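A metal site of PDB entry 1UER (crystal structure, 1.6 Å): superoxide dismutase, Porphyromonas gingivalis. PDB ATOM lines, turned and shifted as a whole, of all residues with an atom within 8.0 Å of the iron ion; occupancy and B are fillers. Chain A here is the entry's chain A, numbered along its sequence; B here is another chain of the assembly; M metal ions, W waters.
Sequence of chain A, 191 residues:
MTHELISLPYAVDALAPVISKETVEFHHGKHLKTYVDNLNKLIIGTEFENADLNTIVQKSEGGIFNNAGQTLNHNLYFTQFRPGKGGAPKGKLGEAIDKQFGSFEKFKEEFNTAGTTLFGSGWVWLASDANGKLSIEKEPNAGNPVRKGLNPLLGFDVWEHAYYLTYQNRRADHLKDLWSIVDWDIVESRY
OD1 of Asp 157 lies within hydrogen-bond range of N of Trp 159 (3.0 Å). ND1 of His 74 lies within hydrogen-bond range of O of Gln 70, 2.7 Å away. O of His 27 lies within hydrogen-bond range of N of Leu 32, 3.0 Å away. OE2 of Glu 160 of chain B is in hydrogen-bond range of ND1 of His 161 (2.9 Å).
Four residues have an atom within 4 Å of the iron ion: His 27, His 74, Asp 157 and His 161. Along chain A the residues within 4 Å of the iron ion span positions 27 to 161.
The iron ion is bound by OD2 of Asp 157 (2.0 Å). Water W1 is bound to the iron ion (2.0 Å). A ring nitrogen (NE2) of His 74 is bound to the iron ion (2.2 Å). A ring nitrogen (NE2) of His 27 binds the iron ion, at 2.2 Å. The iron ion is bound by NE2 of His 161 (2.2 Å). The iron ion has five donor atoms within binding distance.
Water W1 bridges the side-chain carboxylate (OD1) of Asp 157 and the side-chain amide nitrogen (NE2) of Gln 70.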
ATOM      1  N   HIS A  27      13.555  -6.161   2.141  1.00  0.00           N
ATOM      2  CA  HIS A  27      14.755  -5.358   1.977  1.00  0.00           C
ATOM      3  C   HIS A  27      15.132  -5.058   0.536  1.00  0.00           C
ATOM      4  O   HIS A  27      15.337  -3.903   0.165  1.00  0.00           O
ATOM      5  CB  HIS A  27      15.910  -6.021   2.729  1.00  0.00           C
ATOM      6  CG  HIS A  27      17.024  -5.081   3.070  1.00  0.00           C
ATOM      7  ND1 HIS A  27      18.143  -5.498   3.768  1.00  0.00           N
ATOM      8  CD2 HIS A  27      17.217  -3.774   2.796  1.00  0.00           C
ATOM      9  CE1 HIS A  27      18.966  -4.468   3.914  1.00  0.00           C
ATOM     10  NE2 HIS A  27      18.431  -3.418   3.327  1.00  0.00           N
ATOM     11  N   HIS A  28      15.168  -6.107  -0.278  1.00  0.00           N
ATOM     12  CA  HIS A  28      15.494  -5.953  -1.679  1.00  0.00           C
ATOM     13  C   HIS A  28      14.209  -5.617  -2.473  1.00  0.00           C
ATOM     14  O   HIS A  28      14.140  -4.627  -3.220  1.00  0.00           O
ATOM     15  CB  HIS A  28      16.112  -7.264  -2.205  1.00  0.00           C
ATOM     16  CG  HIS A  28      16.373  -7.276  -3.677  1.00  0.00           C
ATOM     17  ND1 HIS A  28      15.461  -7.742  -4.602  1.00  0.00           N
ATOM     18  CD2 HIS A  28      17.459  -6.874  -4.394  1.00  0.00           C
ATOM     19  CE1 HIS A  28      15.969  -7.624  -5.819  1.00  0.00           C
ATOM     20  NE2 HIS A  28      17.176  -7.103  -5.717  1.00  0.00           N
ATOM     21  N   HIS A  31      12.228  -2.043  -0.069  1.00  0.00           N
ATOM     22  CA  HIS A  31      13.111  -0.913   0.226  1.00  0.00           C
ATOM     23  C   HIS A  31      13.987  -0.496  -0.970  1.00  0.00           C
ATOM     24  O   HIS A  31      13.981   0.675  -1.361  1.00  0.00           O
ATOM     25  CB  HIS A  31      14.014  -1.239   1.434  1.00  0.00           C
ATOM     26  CG  HIS A  31      13.284  -1.277   2.744  1.00  0.00           C
ATOM     27  ND1 HIS A  31      13.115  -0.155   3.535  1.00  0.00           N
ATOM     28  CD2 HIS A  31      12.674  -2.300   3.392  1.00  0.00           C
ATOM     29  CE1 HIS A  31      12.404  -0.486   4.609  1.00  0.00           C
ATOM     30  NE2 HIS A  31      12.131  -1.776   4.540  1.00  0.00           N
ATOM     31  N   LEU A  32      14.722  -1.454  -1.541  1.00  0.00           N
ATOM     32  CA  LEU A  32      15.593  -1.111  -2.664  1.00  0.00           C
ATOM     33  C   LEU A  32      14.796  -0.671  -3.876  1.00  0.00           C
ATOM     34  O   LEU A  32      15.191   0.266  -4.544  1.00  0.00           O
ATOM     35  CB  LEU A  32      16.537  -2.283  -3.019  1.00  0.00           C
ATOM     36  CG  LEU A  32      17.602  -1.978  -4.121  1.00  0.00           C
ATOM     37  CD1 LEU A  32      18.345  -0.674  -3.827  1.00  0.00           C
ATOM     38  CD2 LEU A  32      18.594  -3.181  -4.212  1.00  0.00           C
ATOM     39  N   TYR A  35      14.048   2.959  -3.442  1.00  0.00           N
ATOM     40  CA  TYR A  35      15.207   3.820  -3.666  1.00  0.00           C
ATOM     41  C   TYR A  35      15.465   4.004  -5.163  1.00  0.00           C
ATOM     42  O   TYR A  35      15.732   5.120  -5.631  1.00  0.00           O
ATOM     43  CB  TYR A  35      16.453   3.227  -3.028  1.00  0.00           C
ATOM     44  CG  TYR A  35      16.440   3.258  -1.517  1.00  0.00           C
ATOM     45  CD1 TYR A  35      16.139   4.423  -0.821  1.00  0.00           C
ATOM     46  CD2 TYR A  35      16.775   2.111  -0.787  1.00  0.00           C
ATOM     47  CE1 TYR A  35      16.183   4.453   0.605  1.00  0.00           C
ATOM     48  CE2 TYR A  35      16.813   2.128   0.622  1.00  0.00           C
ATOM     49  CZ  TYR A  35      16.523   3.293   1.296  1.00  0.00           C
ATOM     50  OH  TYR A  35      16.596   3.309   2.662  1.00  0.00           O
ATOM     51  N   GLN A  70      21.806   5.132  -1.243  1.00  0.00           N
ATOM     52  CA  GLN A  70      21.198   3.873  -0.812  1.00  0.00           C
ATOM     53  C   GLN A  70      21.198   2.827  -1.943  1.00  0.00           C
ATOM     54  O   GLN A  70      21.426   1.646  -1.689  1.00  0.00           O
ATOM     55  CB  GLN A  70      19.775   4.108  -0.307  1.00  0.00           C
ATOM     56  CG  GLN A  70      19.737   4.658   1.128  1.00  0.00           C
ATOM     57  CD  GLN A  70      20.335   3.701   2.148  1.00  0.00           C
ATOM     58  OE1 GLN A  70      21.550   3.473   2.183  1.00  0.00           O
ATOM     59  NE2 GLN A  70      19.461   3.098   2.975  1.00  0.00           N
ATOM     60  N   ASN A  73      24.858   1.511  -2.081  1.00  0.00           N
ATOM     61  CA  ASN A  73      25.122   0.718  -0.889  1.00  0.00           C
ATOM     62  C   ASN A  73      24.473  -0.671  -1.012  1.00  0.00           C
ATOM     63  O   ASN A  73      25.130  -1.678  -0.759  1.00  0.00           O
ATOM     64  CB  ASN A  73      24.525   1.400   0.349  1.00  0.00           C
ATOM     65  CG  ASN A  73      25.397   2.481   0.902  1.00  0.00           C
ATOM     66  OD1 ASN A  73      26.624   2.366   0.853  1.00  0.00           O
ATOM     67  ND2 ASN A  73      24.791   3.519   1.488  1.00  0.00           N
ATOM     68  N   HIS A  74      23.179  -0.708  -1.370  1.00  0.00           N
ATOM     69  CA  HIS A  74      22.484  -2.000  -1.459  1.00  0.00           C
ATOM     70  C   HIS A  74      22.972  -2.891  -2.604  1.00  0.00           C
ATOM     71  O   HIS A  74      23.025  -4.119  -2.463  1.00  0.00           O
ATOM     72  CB  HIS A  74      20.971  -1.772  -1.525  1.00  0.00           C
ATOM     73  CG  HIS A  74      20.399  -1.354  -0.221  1.00  0.00           C
ATOM     74  ND1 HIS A  74      20.323  -0.036   0.165  1.00  0.00           N
ATOM     75  CD2 HIS A  74      19.858  -2.069   0.798  1.00  0.00           C
ATOM     76  CE1 HIS A  74      19.761   0.045   1.355  1.00  0.00           C
ATOM     77  NE2 HIS A  74      19.469  -1.177   1.768  1.00  0.00           N
ATOM     78  N   TYR A  77      25.964  -4.393  -1.162  1.00  0.00           N
ATOM     79  CA  TYR A  77      25.545  -5.250  -0.055  1.00  0.00           C
ATOM     80  C   TYR A  77      25.031  -6.614  -0.520  1.00  0.00           C
ATOM     81  O   TYR A  77      25.516  -7.639  -0.102  1.00  0.00           O
ATOM     82  CB  TYR A  77      24.466  -4.517   0.712  1.00  0.00           C
ATOM     83  CG  TYR A  77      23.876  -5.246   1.884  1.00  0.00           C
ATOM     84  CD1 TYR A  77      24.567  -5.332   3.101  1.00  0.00           C
ATOM     85  CD2 TYR A  77      22.587  -5.732   1.824  1.00  0.00           C
ATOM     86  CE1 TYR A  77      23.958  -5.879   4.252  1.00  0.00           C
ATOM     87  CE2 TYR A  77      21.969  -6.272   2.944  1.00  0.00           C
ATOM     88  CZ  TYR A  77      22.649  -6.333   4.156  1.00  0.00           C
ATOM     89  OH  TYR A  77      22.002  -6.772   5.300  1.00  0.00           O
ATOM     90  N   PHE A  78      24.035  -6.584  -1.392  1.00  0.00           N
ATOM     91  CA  PHE A  78      23.472  -7.850  -1.847  1.00  0.00           C
ATOM     92  C   PHE A  78      24.424  -8.683  -2.696  1.00  0.00           C
ATOM     93  O   PHE A  78      24.347  -9.932  -2.660  1.00  0.00           O
ATOM     94  CB  PHE A  78      22.173  -7.591  -2.603  1.00  0.00           C
ATOM     95  CG  PHE A  78      21.020  -7.188  -1.686  1.00  0.00           C
ATOM     96  CD1 PHE A  78      20.602  -8.039  -0.674  1.00  0.00           C
ATOM     97  CD2 PHE A  78      20.435  -5.932  -1.813  1.00  0.00           C
ATOM     98  CE1 PHE A  78      19.573  -7.650   0.221  1.00  0.00           C
ATOM     99  CE2 PHE A  78      19.412  -5.530  -0.943  1.00  0.00           C
ATOM    100  CZ  PHE A  78      18.988  -6.403   0.089  1.00  0.00           C
ATOM    101  N   GLY A 122      22.409   3.622   9.309  1.00  0.00           N
ATOM    102  CA  GLY A 122      23.660   3.839   8.609  1.00  0.00           C
ATOM    103  C   GLY A 122      24.332   2.560   8.170  1.00  0.00           C
ATOM    104  O   GLY A 122      23.720   1.491   8.212  1.00  0.00           O
ATOM    105  N   TRP A 123      25.589   2.716   7.750  1.00  0.00           N
ATOM    106  CA  TRP A 123      26.410   1.607   7.222  1.00  0.00           C
ATOM    107  C   TRP A 123      27.809   1.597   7.832  1.00  0.00           C
ATOM    108  O   TRP A 123      28.347   2.675   8.131  1.00  0.00           O
ATOM    109  CB  TRP A 123      26.584   1.792   5.707  1.00  0.00           C
ATOM    110  CG  TRP A 123      25.320   1.618   4.929  1.00  0.00           C
ATOM    111  CD1 TRP A 123      24.281   2.498   4.819  1.00  0.00           C
ATOM    112  CD2 TRP A 123      24.927   0.450   4.203  1.00  0.00           C
ATOM    113  NE1 TRP A 123      23.257   1.951   4.088  1.00  0.00           N
ATOM    114  CE2 TRP A 123      23.628   0.687   3.697  1.00  0.00           C
ATOM    115  CE3 TRP A 123      25.547  -0.796   3.934  1.00  0.00           C
ATOM    116  CZ2 TRP A 123      22.941  -0.244   2.946  1.00  0.00           C
ATOM    117  CZ3 TRP A 123      24.859  -1.726   3.183  1.00  0.00           C
ATOM    118  CH2 TRP A 123      23.556  -1.442   2.694  1.00  0.00           C
ATOM    119  N   ASN A 141      23.151   7.187   7.756  1.00  0.00           N
ATOM    120  CA  ASN A 141      22.066   7.123   6.790  1.00  0.00           C
ATOM    121  C   ASN A 141      22.454   6.568   5.412  1.00  0.00           C
ATOM    122  O   ASN A 141      22.726   5.383   5.338  1.00  0.00           O
ATOM    123  CB  ASN A 141      21.374   8.477   6.676  1.00  0.00           C
ATOM    124  CG  ASN A 141      20.651   8.865   7.957  1.00  0.00           C
ATOM    125  OD1 ASN A 141      20.506   8.055   8.862  1.00  0.00           O
ATOM    126  ND2 ASN A 141      20.192  10.119   8.036  1.00  0.00           N
ATOM    127  N   PHE A 156      28.261  -3.301   5.764  1.00  0.00           N
ATOM    128  CA  PHE A 156      27.184  -3.911   6.550  1.00  0.00           C
ATOM    129  C   PHE A 156      26.146  -2.838   6.839  1.00  0.00           C
ATOM    130  O   PHE A 156      26.470  -1.730   7.280  1.00  0.00           O
ATOM    131  CB  PHE A 156      27.737  -4.467   7.859  1.00  0.00           C
ATOM    132  CG  PHE A 156      28.575  -5.732   7.701  1.00  0.00           C
ATOM    133  CD1 PHE A 156      28.660  -6.376   6.454  1.00  0.00           C
ATOM    134  CD2 PHE A 156      29.280  -6.256   8.798  1.00  0.00           C
ATOM    135  CE1 PHE A 156      29.449  -7.560   6.296  1.00  0.00           C
ATOM    136  CE2 PHE A 156      30.081  -7.448   8.655  1.00  0.00           C
ATOM    137  CZ  PHE A 156      30.154  -8.084   7.394  1.00  0.00           C
ATOM    138  N   ASP A 157      24.891  -3.177   6.571  1.00  0.00           N
ATOM    139  CA  ASP A 157      23.746  -2.292   6.728  1.00  0.00           C
ATOM    140  C   ASP A 157      23.286  -2.362   8.170  1.00  0.00           C
ATOM    141  O   ASP A 157      22.947  -3.459   8.648  1.00  0.00           O
ATOM    142  CB  ASP A 157      22.637  -2.770   5.811  1.00  0.00           C
ATOM    143  CG  ASP A 157      21.479  -1.810   5.686  1.00  0.00           C
ATOM    144  OD1 ASP A 157      21.476  -0.753   6.338  1.00  0.00           O
ATOM    145  OD2 ASP A 157      20.558  -2.107   4.890  1.00  0.00           O
ATOM    146  N   VAL A 158      23.282  -1.233   8.878  1.00  0.00           N
ATOM    147  CA  VAL A 158      22.811  -1.252  10.247  1.00  0.00           C
ATOM    148  C   VAL A 158      21.489  -0.490  10.387  1.00  0.00           C
ATOM    149  O   VAL A 158      21.031  -0.224  11.504  1.00  0.00           O
ATOM    150  CB  VAL A 158      23.878  -0.801  11.320  1.00  0.00           C
ATOM    151  CG1 VAL A 158      25.110  -1.785  11.276  1.00  0.00           C
ATOM    152  CG2 VAL A 158      24.339   0.615  11.065  1.00  0.00           C
ATOM    153  N   TRP A 159      20.865  -0.134   9.258  1.00  0.00           N
ATOM    154  CA  TRP A 159      19.485   0.395   9.326  1.00  0.00           C
ATOM    155  C   TRP A 159      18.712  -0.772   9.951  1.00  0.00           C
ATOM    156  O   TRP A 159      18.958  -1.933   9.605  1.00  0.00           O
ATOM    157  CB  TRP A 159      18.941   0.643   7.934  1.00  0.00           C
ATOM    158  CG  TRP A 159      19.430   1.943   7.327  1.00  0.00           C
ATOM    159  CD1 TRP A 159      20.722   2.278   6.995  1.00  0.00           C
ATOM    160  CD2 TRP A 159      18.593   3.001   6.883  1.00  0.00           C
ATOM    161  NE1 TRP A 159      20.716   3.506   6.332  1.00  0.00           N
ATOM    162  CE2 TRP A 159      19.425   3.966   6.252  1.00  0.00           C
ATOM    163  CE3 TRP A 159      17.213   3.231   6.936  1.00  0.00           C
ATOM    164  CZ2 TRP A 159      18.907   5.146   5.697  1.00  0.00           C
ATOM    165  CZ3 TRP A 159      16.683   4.419   6.367  1.00  0.00           C
ATOM    166  CH2 TRP A 159      17.559   5.351   5.752  1.00  0.00           C
ATOM    167  N   GLU A 160      17.771  -0.493  10.855  1.00  0.00           N
ATOM    168  CA  GLU A 160      17.024  -1.582  11.503  1.00  0.00           C
ATOM    169  C   GLU A 160      16.281  -2.510  10.561  1.00  0.00           C
ATOM    170  O   GLU A 160      16.130  -3.697  10.885  1.00  0.00           O
ATOM    171  CB  GLU A 160      16.096  -1.017  12.614  1.00  0.00           C
ATOM    172  CG  GLU A 160      16.941  -0.504  13.811  1.00  0.00           C
ATOM    173  CD  GLU A 160      16.148   0.251  14.882  1.00  0.00           C
ATOM    174  OE1 GLU A 160      15.248   1.076  14.535  1.00  0.00           O
ATOM    175  OE2 GLU A 160      16.467   0.026  16.074  1.00  0.00           O
ATOM    176  N   HIS A 161      15.805  -2.017   9.406  1.00  0.00           N
ATOM    177  CA  HIS A 161      15.098  -2.911   8.483  1.00  0.00           C
ATOM    178  C   HIS A 161      15.999  -4.061   8.007  1.00  0.00           C
ATOM    179  O   HIS A 161      15.504  -5.077   7.530  1.00  0.00           O
ATOM    180  CB  HIS A 161      14.510  -2.168   7.251  1.00  0.00           C
ATOM    181  CG  HIS A 161      15.528  -1.489   6.383  1.00  0.00           C
ATOM    182  ND1 HIS A 161      15.517  -0.134   6.155  1.00  0.00           N
ATOM    183  CD2 HIS A 161      16.567  -1.988   5.667  1.00  0.00           C
ATOM    184  CE1 HIS A 161      16.514   0.182   5.348  1.00  0.00           C
ATOM    185  NE2 HIS A 161      17.166  -0.912   5.029  1.00  0.00           N
ATOM    186  N   ALA A 162      17.324  -3.927   8.147  1.00  0.00           N
ATOM    187  CA  ALA A 162      18.220  -5.003   7.702  1.00  0.00           C
ATOM    188  C   ALA A 162      18.208  -6.248   8.565  1.00  0.00           C
ATOM    189  O   ALA A 162      18.516  -7.344   8.096  1.00  0.00           O
ATOM    190  CB  ALA A 162      19.679  -4.471   7.587  1.00  0.00           C
ATOM    191  N   TYR A 163      17.790  -6.088   9.813  1.00  0.00           N
ATOM    192  CA  TYR A 163      17.843  -7.206  10.751  1.00  0.00           C
ATOM    193  C   TYR A 163      16.694  -7.281  11.729  1.00  0.00           C
ATOM    194  O   TYR A 163      16.655  -8.244  12.493  1.00  0.00           O
ATOM    195  CB  TYR A 163      19.140  -7.108  11.585  1.00  0.00           C
ATOM    196  CG  TYR A 163      19.292  -5.812  12.376  1.00  0.00           C
ATOM    197  CD1 TYR A 163      18.686  -5.643  13.637  1.00  0.00           C
ATOM    198  CD2 TYR A 163      20.074  -4.763  11.886  1.00  0.00           C
ATOM    199  CE1 TYR A 163      18.852  -4.473  14.388  1.00  0.00           C
ATOM    200  CE2 TYR A 163      20.252  -3.566  12.629  1.00  0.00           C
ATOM    201  CZ  TYR A 163      19.637  -3.436  13.876  1.00  0.00           C
ATOM    202  OH  TYR A 163      19.817  -2.284  14.619  1.00  0.00           O
ATOM    203  N   GLU B 160      12.769   2.780  12.766  1.00  0.00           N
ATOM    204  CA  GLU B 160      12.113   1.548  12.292  1.00  0.00           C
ATOM    205  C   GLU B 160      11.694   0.558  13.393  1.00  0.00           C
ATOM    206  O   GLU B 160      10.678  -0.151  13.230  1.00  0.00           O
ATOM    207  CB  GLU B 160      12.979   0.880  11.227  1.00  0.00           C
ATOM    208  CG  GLU B 160      12.965   1.695   9.922  1.00  0.00           C
ATOM    209  CD  GLU B 160      13.872   1.155   8.828  1.00  0.00           C
ATOM    210  OE1 GLU B 160      15.020   0.727   9.149  1.00  0.00           O
ATOM    211  OE2 GLU B 160      13.442   1.163   7.642  1.00  0.00           O
HETATM  212 FE    FE M   1      19.036  -1.343   3.885  1.00  0.00          FE
HETATM  213  O   HOH W   1      19.620   0.528   4.483  1.00  0.00           O
